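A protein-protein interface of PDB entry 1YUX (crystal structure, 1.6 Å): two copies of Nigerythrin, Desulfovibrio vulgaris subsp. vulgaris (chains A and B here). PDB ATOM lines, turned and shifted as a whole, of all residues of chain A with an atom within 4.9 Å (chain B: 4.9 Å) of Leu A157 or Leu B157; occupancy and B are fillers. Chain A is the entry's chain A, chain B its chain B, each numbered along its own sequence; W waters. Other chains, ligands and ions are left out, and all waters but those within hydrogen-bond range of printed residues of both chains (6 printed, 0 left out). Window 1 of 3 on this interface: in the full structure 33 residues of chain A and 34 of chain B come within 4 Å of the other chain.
Ile A109 touches Ile B116, and with the chains exchanged Ile A116 touches Ile B109. Glu A154 touches Asn B161, and with the chains exchanged Asn A161 touches Glu B154. Leu A157 touches Glu B154, but with the chains exchanged Glu A154 does not touch Leu B157 (4.02 Å). Leu A157 touches its own counterpart, Leu B157. Of the 14 pairs that touch across the chains among the printed residues, 10 have their exchanged pair printed and touching as well.
The side-chain carboxylate (OE2) of Glu A154 sits at hydrogen-bond distance from the side-chain amide nitrogen (ND2) of Asn B161, 2.8 Å away. The side-chain hydroxyl of Ser B150 sits at hydrogen-bond distance from the side-chain amide oxygen of Asn A161, at 2.6 Å. The side-chain amide nitrogen (ND2) of Asn A161 lies within hydrogen-bond range of the side-chain carboxylate (OE2) of Glu B154 (2.8 Å).
Ile B116 touches Ile A109 (CG2 to CG2, 3.7 Å). Ile A116 touches Ile B109 (CG2 to CG2, 3.8 Å). Ile B116 touches Ile A116 (CD1 to CD1, 3.5 Å). Ala A153 touches Leu B157. Glu A154 touches Ala B158. Ser B150 touches Leu A157. CB of Ala B153 touches CD1 of Leu A157, at 3.7 Å. Leu A157 touches Glu B154. CA of Ala A158 touches OE2 of Glu B154, at 3.4 Å. Tyr A160 touches Ser B150.
Of the printed residues of chain B, Leu A157 touches Ser B150 (3.8 Å), Ala B153 (3.7 Å), Glu B154 (3.98 Å) and Leu B157 (3.8 Å). Leu B157 touches just these residues of chain A: Ala A153 (3.8 Å) and Leu A157 (3.8 Å). Of the printed residues of chain A, Ile B109 touches Ile A116. Of the printed residues of chain A, Ala B153 touches Leu A157 (3.7 Å). Of the printed residues of chain B, Asn A161 touches Ser B150 and Glu B154. Ala A112 touches none of the printed residues of chain B. The nearest printed residue of chain A that does not touch Ser B150 is Ile A109 (6.2 Å).
Of the 13 printed residues of chain B, 8 touch a printed residue of chain A. Hydrophobic or aromatic side chains of chain B within 4 Å of the printed part of chain A: Ile B109, Ile B116, Ala B153, Leu B157 and Ala B158. Hydrophobic or aromatic side chains of chain A within 4 Å of the printed part of chain B: Ile A109, Ile A116, Leu A157, Ala A158 and Tyr A160. Among the printed residues, 14 pairs touch across the chains. Among the printed residues, no Asp or Glu carboxylate lies within 4 Å of a Lys or Arg side-chain nitrogen of the other chain.
The side-chain carboxylate (OE1) of Glu A154 lies within salt-bridge range of the guanidinium group (NH2) of Arg A155. The backbone carbonyl oxygen of Leu A157 sits at hydrogen-bond distance from the side-chain amide nitrogen of Asn A161. The guanidinium group of Arg B155 is in salt-bridge range of the side-chain carboxylate of Glu B154 (3.7 Å). The backbone carbonyl oxygen of Leu B157 lies within hydrogen-bond range of the side-chain amide nitrogen of Asn B161.
Water W4 bridges the side-chain carboxylate of Glu A154 (2.5 Å) and the side-chain amide nitrogen of Asn B161 (3.2 Å). Water W5 lies within hydrogen-bond range of the side-chain carboxylate of Glu A154 (2.5 Å), the side-chain carboxylate of Glu B154 (2.6 Å), the guanidinium group of Arg B155 (3.3 Å) and the guanidinium group of Arg A155 (3.5 Å). Water W3 bridges the side-chain carboxylate (OE2) of Glu B154 and the side-chain amide nitrogen (ND2) of Asn A161. Water W2 bridges O of Ala A158 (2.7 Å) and OE2 of Glu B154 (3.5 Å). Water W6 bridges the backbone carbonyl oxygen of Ala B158 (2.8 Å) and the side-chain carboxylate of Glu A154 (3.3 Å). Water W1 lies within hydrogen-bond range of the side-chain hydroxyl of Ser B150 and the side-chain amide oxygen of Asn A161.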
ATOM      1  N   ILE A 109     -28.177   0.757  -6.552  1.00  0.00           N
ATOM      2  CA  ILE A 109     -29.238  -0.241  -6.526  1.00  0.00           C
ATOM      3  C   ILE A 109     -29.477  -0.784  -7.934  1.00  0.00           C
ATOM      4  O   ILE A 109     -29.666  -1.985  -8.120  1.00  0.00           O
ATOM      5  CB  ILE A 109     -30.552   0.360  -5.980  1.00  0.00           C
ATOM      6  CG1 ILE A 109     -30.395   0.684  -4.493  1.00  0.00           C
ATOM      7  CG2 ILE A 109     -31.714  -0.609  -6.209  1.00  0.00           C
ATOM      8  CD1 ILE A 109     -30.224  -0.537  -3.599  1.00  0.00           C
ATOM      9  N   ALA A 112     -26.724  -3.109  -8.605  1.00  0.00           N
ATOM     10  CA  ALA A 112     -26.926  -4.343  -7.855  1.00  0.00           C
ATOM     11  C   ALA A 112     -27.967  -5.229  -8.525  1.00  0.00           C
ATOM     12  O   ALA A 112     -27.764  -6.435  -8.679  1.00  0.00           O
ATOM     13  CB  ALA A 112     -27.355  -4.020  -6.430  1.00  0.00           C
ATOM     14  N   ILE A 116     -27.385  -8.960 -10.050  1.00  0.00           N
ATOM     15  CA  ILE A 116     -28.140 -10.103  -9.566  1.00  0.00           C
ATOM     16  C   ILE A 116     -28.783 -10.829 -10.745  1.00  0.00           C
ATOM     17  O   ILE A 116     -28.795 -12.057 -10.795  1.00  0.00           O
ATOM     18  CB  ILE A 116     -29.201  -9.655  -8.544  1.00  0.00           C
ATOM     19  CG1 ILE A 116     -28.489  -9.201  -7.265  1.00  0.00           C
ATOM     20  CG2 ILE A 116     -30.179 -10.792  -8.257  1.00  0.00           C
ATOM     21  CD1 ILE A 116     -29.391  -8.578  -6.232  1.00  0.00           C
ATOM     22  N   ALA A 153     -22.466  -7.374  -7.103  1.00  0.00           N
ATOM     23  CA  ALA A 153     -23.722  -7.067  -6.435  1.00  0.00           C
ATOM     24  C   ALA A 153     -23.451  -6.741  -4.973  1.00  0.00           C
ATOM     25  O   ALA A 153     -23.945  -5.746  -4.443  1.00  0.00           O
ATOM     26  CB  ALA A 153     -24.685  -8.245  -6.546  1.00  0.00           C
ATOM     27  N   GLU A 154     -22.651  -7.574  -4.322  1.00  0.00           N
ATOM     28  CA  GLU A 154     -22.333  -7.341  -2.925  1.00  0.00           C
ATOM     29  C   GLU A 154     -21.566  -6.029  -2.742  1.00  0.00           C
ATOM     30  O   GLU A 154     -21.832  -5.282  -1.802  1.00  0.00           O
ATOM     31  CB  GLU A 154     -21.522  -8.505  -2.356  1.00  0.00           C
ATOM     32  CG  GLU A 154     -21.256  -8.322  -0.874  1.00  0.00           C
ATOM     33  CD  GLU A 154     -20.468  -9.453  -0.255  1.00  0.00           C
ATOM     34  OE1 GLU A 154     -19.986  -9.264   0.878  1.00  0.00           O
ATOM     35  OE2 GLU A 154     -20.339 -10.521  -0.886  1.00  0.00           O
ATOM     36  N   ARG A 155     -20.614  -5.749  -3.627  1.00  0.00           N
ATOM     37  CA  ARG A 155     -19.854  -4.507  -3.523  1.00  0.00           C
ATOM     38  C   ARG A 155     -20.781  -3.304  -3.633  1.00  0.00           C
ATOM     39  O   ARG A 155     -20.617  -2.314  -2.919  1.00  0.00           O
ATOM     40  CB  ARG A 155     -18.783  -4.420  -4.614  1.00  0.00           C
ATOM     41  CG  ARG A 155     -17.555  -5.296  -4.389  1.00  0.00           C
ATOM     42  CD  ARG A 155     -16.848  -4.941  -3.087  1.00  0.00           C
ATOM     43  NE  ARG A 155     -17.304  -5.779  -1.979  1.00  0.00           N
ATOM     44  CZ  ARG A 155     -17.457  -5.361  -0.726  1.00  0.00           C
ATOM     45  NH1 ARG A 155     -17.199  -4.100  -0.397  1.00  0.00           N
ATOM     46  NH2 ARG A 155     -17.853  -6.216   0.210  1.00  0.00           N
ATOM     47  N   TYR A 156     -21.757  -3.383  -4.531  1.00  0.00           N
ATOM     48  CA  TYR A 156     -22.691  -2.282  -4.703  1.00  0.00           C
ATOM     49  C   TYR A 156     -23.567  -2.094  -3.469  1.00  0.00           C
ATOM     50  O   TYR A 156     -23.806  -0.965  -3.044  1.00  0.00           O
ATOM     51  CB  TYR A 156     -23.550  -2.511  -5.950  1.00  0.00           C
ATOM     52  CG  TYR A 156     -22.832  -2.199  -7.247  1.00  0.00           C
ATOM     53  CD1 TYR A 156     -23.194  -2.836  -8.433  1.00  0.00           C
ATOM     54  CD2 TYR A 156     -21.831  -1.226  -7.302  1.00  0.00           C
ATOM     55  CE1 TYR A 156     -22.585  -2.513  -9.639  1.00  0.00           C
ATOM     56  CE2 TYR A 156     -21.215  -0.894  -8.506  1.00  0.00           C
ATOM     57  CZ  TYR A 156     -21.599  -1.539  -9.668  1.00  0.00           C
ATOM     58  OH  TYR A 156     -21.010  -1.200 -10.868  1.00  0.00           O
ATOM     59  N   LEU A 157     -24.049  -3.188  -2.889  1.00  0.00           N
ATOM     60  CA  LEU A 157     -24.873  -3.068  -1.691  1.00  0.00           C
ATOM     61  C   LEU A 157     -24.041  -2.549  -0.523  1.00  0.00           C
ATOM     62  O   LEU A 157     -24.535  -1.778   0.296  1.00  0.00           O
ATOM     63  CB  LEU A 157     -25.503  -4.413  -1.319  1.00  0.00           C
ATOM     64  CG  LEU A 157     -26.981  -4.585  -1.685  1.00  0.00           C
ATOM     65  CD1 LEU A 157     -27.813  -3.555  -0.946  1.00  0.00           C
ATOM     66  CD2 LEU A 157     -27.173  -4.439  -3.174  1.00  0.00           C
ATOM     67  N   ALA A 158     -22.781  -2.970  -0.446  1.00  0.00           N
ATOM     68  CA  ALA A 158     -21.905  -2.519   0.630  1.00  0.00           C
ATOM     69  C   ALA A 158     -21.700  -1.010   0.522  1.00  0.00           C
ATOM     70  O   ALA A 158     -21.732  -0.297   1.524  1.00  0.00           O
ATOM     71  CB  ALA A 158     -20.568  -3.236   0.559  1.00  0.00           C
ATOM     72  N   ALA A 159     -21.501  -0.531  -0.701  1.00  0.00           N
ATOM     73  CA  ALA A 159     -21.294   0.891  -0.940  1.00  0.00           C
ATOM     74  C   ALA A 159     -22.561   1.670  -0.594  1.00  0.00           C
ATOM     75  O   ALA A 159     -22.500   2.764  -0.033  1.00  0.00           O
ATOM     76  CB  ALA A 159     -20.910   1.120  -2.396  1.00  0.00           C
ATOM     77  N   TYR A 160     -23.707   1.092  -0.930  1.00  0.00           N
ATOM     78  CA  TYR A 160     -24.998   1.704  -0.654  1.00  0.00           C
ATOM     79  C   TYR A 160     -25.190   1.841   0.858  1.00  0.00           C
ATOM     80  O   TYR A 160     -25.596   2.889   1.356  1.00  0.00           O
ATOM     81  CB  TYR A 160     -26.099   0.824  -1.246  1.00  0.00           C
ATOM     82  CG  TYR A 160     -27.513   1.326  -1.076  1.00  0.00           C
ATOM     83  CD1 TYR A 160     -28.105   2.155  -2.035  1.00  0.00           C
ATOM     84  CD2 TYR A 160     -28.288   0.910   0.006  1.00  0.00           C
ATOM     85  CE1 TYR A 160     -29.442   2.543  -1.921  1.00  0.00           C
ATOM     86  CE2 TYR A 160     -29.617   1.289   0.130  1.00  0.00           C
ATOM     87  CZ  TYR A 160     -30.191   2.100  -0.839  1.00  0.00           C
ATOM     88  OH  TYR A 160     -31.526   2.417  -0.738  1.00  0.00           O
ATOM     89  N   ASN A 161     -24.881   0.779   1.593  1.00  0.00           N
ATOM     90  CA  ASN A 161     -25.046   0.809   3.042  1.00  0.00           C
ATOM     91  C   ASN A 161     -24.146   1.819   3.741  1.00  0.00           C
ATOM     92  O   ASN A 161     -24.506   2.349   4.794  1.00  0.00           O
ATOM     93  CB  ASN A 161     -24.830  -0.588   3.630  1.00  0.00           C
ATOM     94  CG  ASN A 161     -25.967  -1.525   3.300  1.00  0.00           C
ATOM     95  OD1 ASN A 161     -27.101  -1.087   3.139  1.00  0.00           O
ATOM     96  ND2 ASN A 161     -25.680  -2.818   3.211  1.00  0.00           N
ATOM     97  N   ILE B 109     -31.147 -15.333  -3.275  1.00  0.00           N
ATOM     98  CA  ILE B 109     -31.373 -14.314  -4.295  1.00  0.00           C
ATOM     99  C   ILE B 109     -32.773 -13.733  -4.120  1.00  0.00           C
ATOM    100  O   ILE B 109     -32.971 -12.522  -4.223  1.00  0.00           O
ATOM    101  CB  ILE B 109     -31.218 -14.905  -5.716  1.00  0.00           C
ATOM    102  CG1 ILE B 109     -29.747 -15.244  -5.978  1.00  0.00           C
ATOM    103  CG2 ILE B 109     -31.739 -13.920  -6.758  1.00  0.00           C
ATOM    104  CD1 ILE B 109     -28.804 -14.037  -5.975  1.00  0.00           C
ATOM    105  N   ALA B 112     -32.546 -11.407  -1.264  1.00  0.00           N
ATOM    106  CA  ALA B 112     -31.851 -10.180  -1.633  1.00  0.00           C
ATOM    107  C   ALA B 112     -32.746  -9.259  -2.449  1.00  0.00           C
ATOM    108  O   ALA B 112     -32.791  -8.052  -2.210  1.00  0.00           O
ATOM    109  CB  ALA B 112     -30.591 -10.509  -2.422  1.00  0.00           C
ATOM    110  N   ILE B 116     -33.949  -5.576  -1.409  1.00  0.00           N
ATOM    111  CA  ILE B 116     -33.641  -4.422  -2.234  1.00  0.00           C
ATOM    112  C   ILE B 116     -34.918  -3.648  -2.549  1.00  0.00           C
ATOM    113  O   ILE B 116     -34.935  -2.416  -2.503  1.00  0.00           O
ATOM    114  CB  ILE B 116     -32.938  -4.855  -3.529  1.00  0.00           C
ATOM    115  CG1 ILE B 116     -31.528  -5.352  -3.187  1.00  0.00           C
ATOM    116  CG2 ILE B 116     -32.889  -3.693  -4.514  1.00  0.00           C
ATOM    117  CD1 ILE B 116     -30.804  -6.018  -4.338  1.00  0.00           C
ATOM    118  N   SER B 150     -31.443  -2.915   3.685  1.00  0.00           N
ATOM    119  CA  SER B 150     -30.282  -2.908   2.804  1.00  0.00           C
ATOM    120  C   SER B 150     -29.146  -3.733   3.418  1.00  0.00           C
ATOM    121  O   SER B 150     -28.334  -4.310   2.698  1.00  0.00           O
ATOM    122  CB  SER B 150     -29.838  -1.472   2.500  1.00  0.00           C
ATOM    123  OG  SER B 150     -29.610  -0.731   3.682  1.00  0.00           O
ATOM    124  N   ALA B 153     -29.985  -7.245   2.614  1.00  0.00           N
ATOM    125  CA  ALA B 153     -29.656  -7.512   1.222  1.00  0.00           C
ATOM    126  C   ALA B 153     -28.186  -7.883   1.107  1.00  0.00           C
ATOM    127  O   ALA B 153     -27.838  -8.865   0.452  1.00  0.00           O
ATOM    128  CB  ALA B 153     -29.951  -6.286   0.360  1.00  0.00           C
ATOM    129  N   GLU B 154     -27.323  -7.097   1.746  1.00  0.00           N
ATOM    130  CA  GLU B 154     -25.895  -7.373   1.683  1.00  0.00           C
ATOM    131  C   GLU B 154     -25.555  -8.709   2.340  1.00  0.00           C
ATOM    132  O   GLU B 154     -24.746  -9.471   1.814  1.00  0.00           O
ATOM    133  CB  GLU B 154     -25.088  -6.248   2.343  1.00  0.00           C
ATOM    134  CG  GLU B 154     -23.589  -6.507   2.290  1.00  0.00           C
ATOM    135  CD  GLU B 154     -22.753  -5.386   2.859  1.00  0.00           C
ATOM    136  OE1 GLU B 154     -21.536  -5.604   3.039  1.00  0.00           O
ATOM    137  OE2 GLU B 154     -23.295  -4.293   3.121  1.00  0.00           O
ATOM    138  N   ARG B 155     -26.175  -8.999   3.478  1.00  0.00           N
ATOM    139  CA  ARG B 155     -25.907 -10.259   4.163  1.00  0.00           C
ATOM    140  C   ARG B 155     -26.271 -11.449   3.278  1.00  0.00           C
ATOM    141  O   ARG B 155     -25.553 -12.450   3.240  1.00  0.00           O
ATOM    142  CB  ARG B 155     -26.692 -10.339   5.479  1.00  0.00           C
ATOM    143  CG  ARG B 155     -26.097  -9.535   6.625  1.00  0.00           C
ATOM    144  CD  ARG B 155     -24.662  -9.964   6.897  1.00  0.00           C
ATOM    145  NE  ARG B 155     -23.702  -9.098   6.218  1.00  0.00           N
ATOM    146  CZ  ARG B 155     -22.524  -9.493   5.747  1.00  0.00           C
ATOM    147  NH1 ARG B 155     -22.135 -10.760   5.858  1.00  0.00           N
ATOM    148  NH2 ARG B 155     -21.720  -8.609   5.179  1.00  0.00           N
ATOM    149  N   TYR B 156     -27.389 -11.336   2.566  1.00  0.00           N
ATOM    150  CA  TYR B 156     -27.837 -12.409   1.687  1.00  0.00           C
ATOM    151  C   TYR B 156     -26.883 -12.597   0.516  1.00  0.00           C
ATOM    152  O   TYR B 156     -26.585 -13.722   0.125  1.00  0.00           O
ATOM    153  CB  TYR B 156     -29.247 -12.115   1.173  1.00  0.00           C
ATOM    154  CG  TYR B 156     -30.348 -12.398   2.176  1.00  0.00           C
ATOM    155  CD1 TYR B 156     -31.542 -11.677   2.145  1.00  0.00           C
ATOM    156  CD2 TYR B 156     -30.221 -13.426   3.118  1.00  0.00           C
ATOM    157  CE1 TYR B 156     -32.585 -11.970   3.020  1.00  0.00           C
ATOM    158  CE2 TYR B 156     -31.260 -13.730   3.999  1.00  0.00           C
ATOM    159  CZ  TYR B 156     -32.439 -13.001   3.941  1.00  0.00           C
ATOM    160  OH  TYR B 156     -33.484 -13.328   4.774  1.00  0.00           O
ATOM    161  N   LEU B 157     -26.398 -11.494  -0.042  1.00  0.00           N
ATOM    162  CA  LEU B 157     -25.474 -11.590  -1.161  1.00  0.00           C
ATOM    163  C   LEU B 157     -24.140 -12.158  -0.683  1.00  0.00           C
ATOM    164  O   LEU B 157     -23.510 -12.949  -1.385  1.00  0.00           O
ATOM    165  CB  LEU B 157     -25.278 -10.214  -1.804  1.00  0.00           C
ATOM    166  CG  LEU B 157     -26.571  -9.653  -2.403  1.00  0.00           C
ATOM    167  CD1 LEU B 157     -26.388  -8.198  -2.799  1.00  0.00           C
ATOM    168  CD2 LEU B 157     -26.981 -10.495  -3.596  1.00  0.00           C
ATOM    169  N   ALA B 158     -23.720 -11.773   0.518  1.00  0.00           N
ATOM    170  CA  ALA B 158     -22.466 -12.277   1.066  1.00  0.00           C
ATOM    171  C   ALA B 158     -22.579 -13.785   1.272  1.00  0.00           C
ATOM    172  O   ALA B 158     -21.647 -14.534   0.978  1.00  0.00           O
ATOM    173  CB  ALA B 158     -22.159 -11.595   2.388  1.00  0.00           C
ATOM    174  N   ALA B 159     -23.728 -14.227   1.770  1.00  0.00           N
ATOM    175  CA  ALA B 159     -23.941 -15.649   2.010  1.00  0.00           C
ATOM    176  C   ALA B 159     -23.967 -16.396   0.687  1.00  0.00           C
ATOM    177  O   ALA B 159     -23.479 -17.521   0.587  1.00  0.00           O
ATOM    178  CB  ALA B 159     -25.244 -15.862   2.759  1.00  0.00           C
ATOM    179  N   TYR B 160     -24.542 -15.761  -0.329  1.00  0.00           N
ATOM    180  CA  TYR B 160     -24.634 -16.355  -1.657  1.00  0.00           C
ATOM    181  C   TYR B 160     -23.235 -16.527  -2.245  1.00  0.00           C
ATOM    182  O   TYR B 160     -22.897 -17.578  -2.780  1.00  0.00           O
ATOM    183  CB  TYR B 160     -25.469 -15.443  -2.558  1.00  0.00           C
ATOM    184  CG  TYR B 160     -25.660 -15.934  -3.975  1.00  0.00           C
ATOM    185  CD1 TYR B 160     -26.730 -16.761  -4.310  1.00  0.00           C
ATOM    186  CD2 TYR B 160     -24.804 -15.516  -4.992  1.00  0.00           C
ATOM    187  CE1 TYR B 160     -26.950 -17.152  -5.635  1.00  0.00           C
ATOM    188  CE2 TYR B 160     -25.012 -15.901  -6.313  1.00  0.00           C
ATOM    189  CZ  TYR B 160     -26.087 -16.713  -6.627  1.00  0.00           C
ATOM    190  OH  TYR B 160     -26.315 -17.061  -7.936  1.00  0.00           O
ATOM    191  N   ASN B 161     -22.417 -15.489  -2.127  1.00  0.00           N
ATOM    192  CA  ASN B 161     -21.063 -15.537  -2.660  1.00  0.00           C
ATOM    193  C   ASN B 161     -20.200 -16.591  -1.987  1.00  0.00           C
ATOM    194  O   ASN B 161     -19.341 -17.190  -2.628  1.00  0.00           O
ATOM    195  CB  ASN B 161     -20.405 -14.163  -2.550  1.00  0.00           C
ATOM    196  CG  ASN B 161     -20.963 -13.194  -3.552  1.00  0.00           C
ATOM    197  OD1 ASN B 161     -21.384 -13.603  -4.626  1.00  0.00           O
ATOM    198  ND2 ASN B 161     -20.965 -11.910  -3.220  1.00  0.00           N
HETATM  199  O   HOH W   1     -28.275   0.464   5.968  1.00  0.00           O
HETATM  200  O   HOH W   2     -21.319  -1.514   3.878  1.00  0.00           O
HETATM  201  O   HOH W   3     -23.163  -2.920   5.396  1.00  0.00           O
HETATM  202  O   HOH W   4     -18.280 -11.920  -1.416  1.00  0.00           O
HETATM  203  O   HOH W   5     -19.819  -7.538   2.744  1.00  0.00           O
HETATM  204  O   HOH W   6     -19.198 -13.238   0.665  1.00  0.00           O
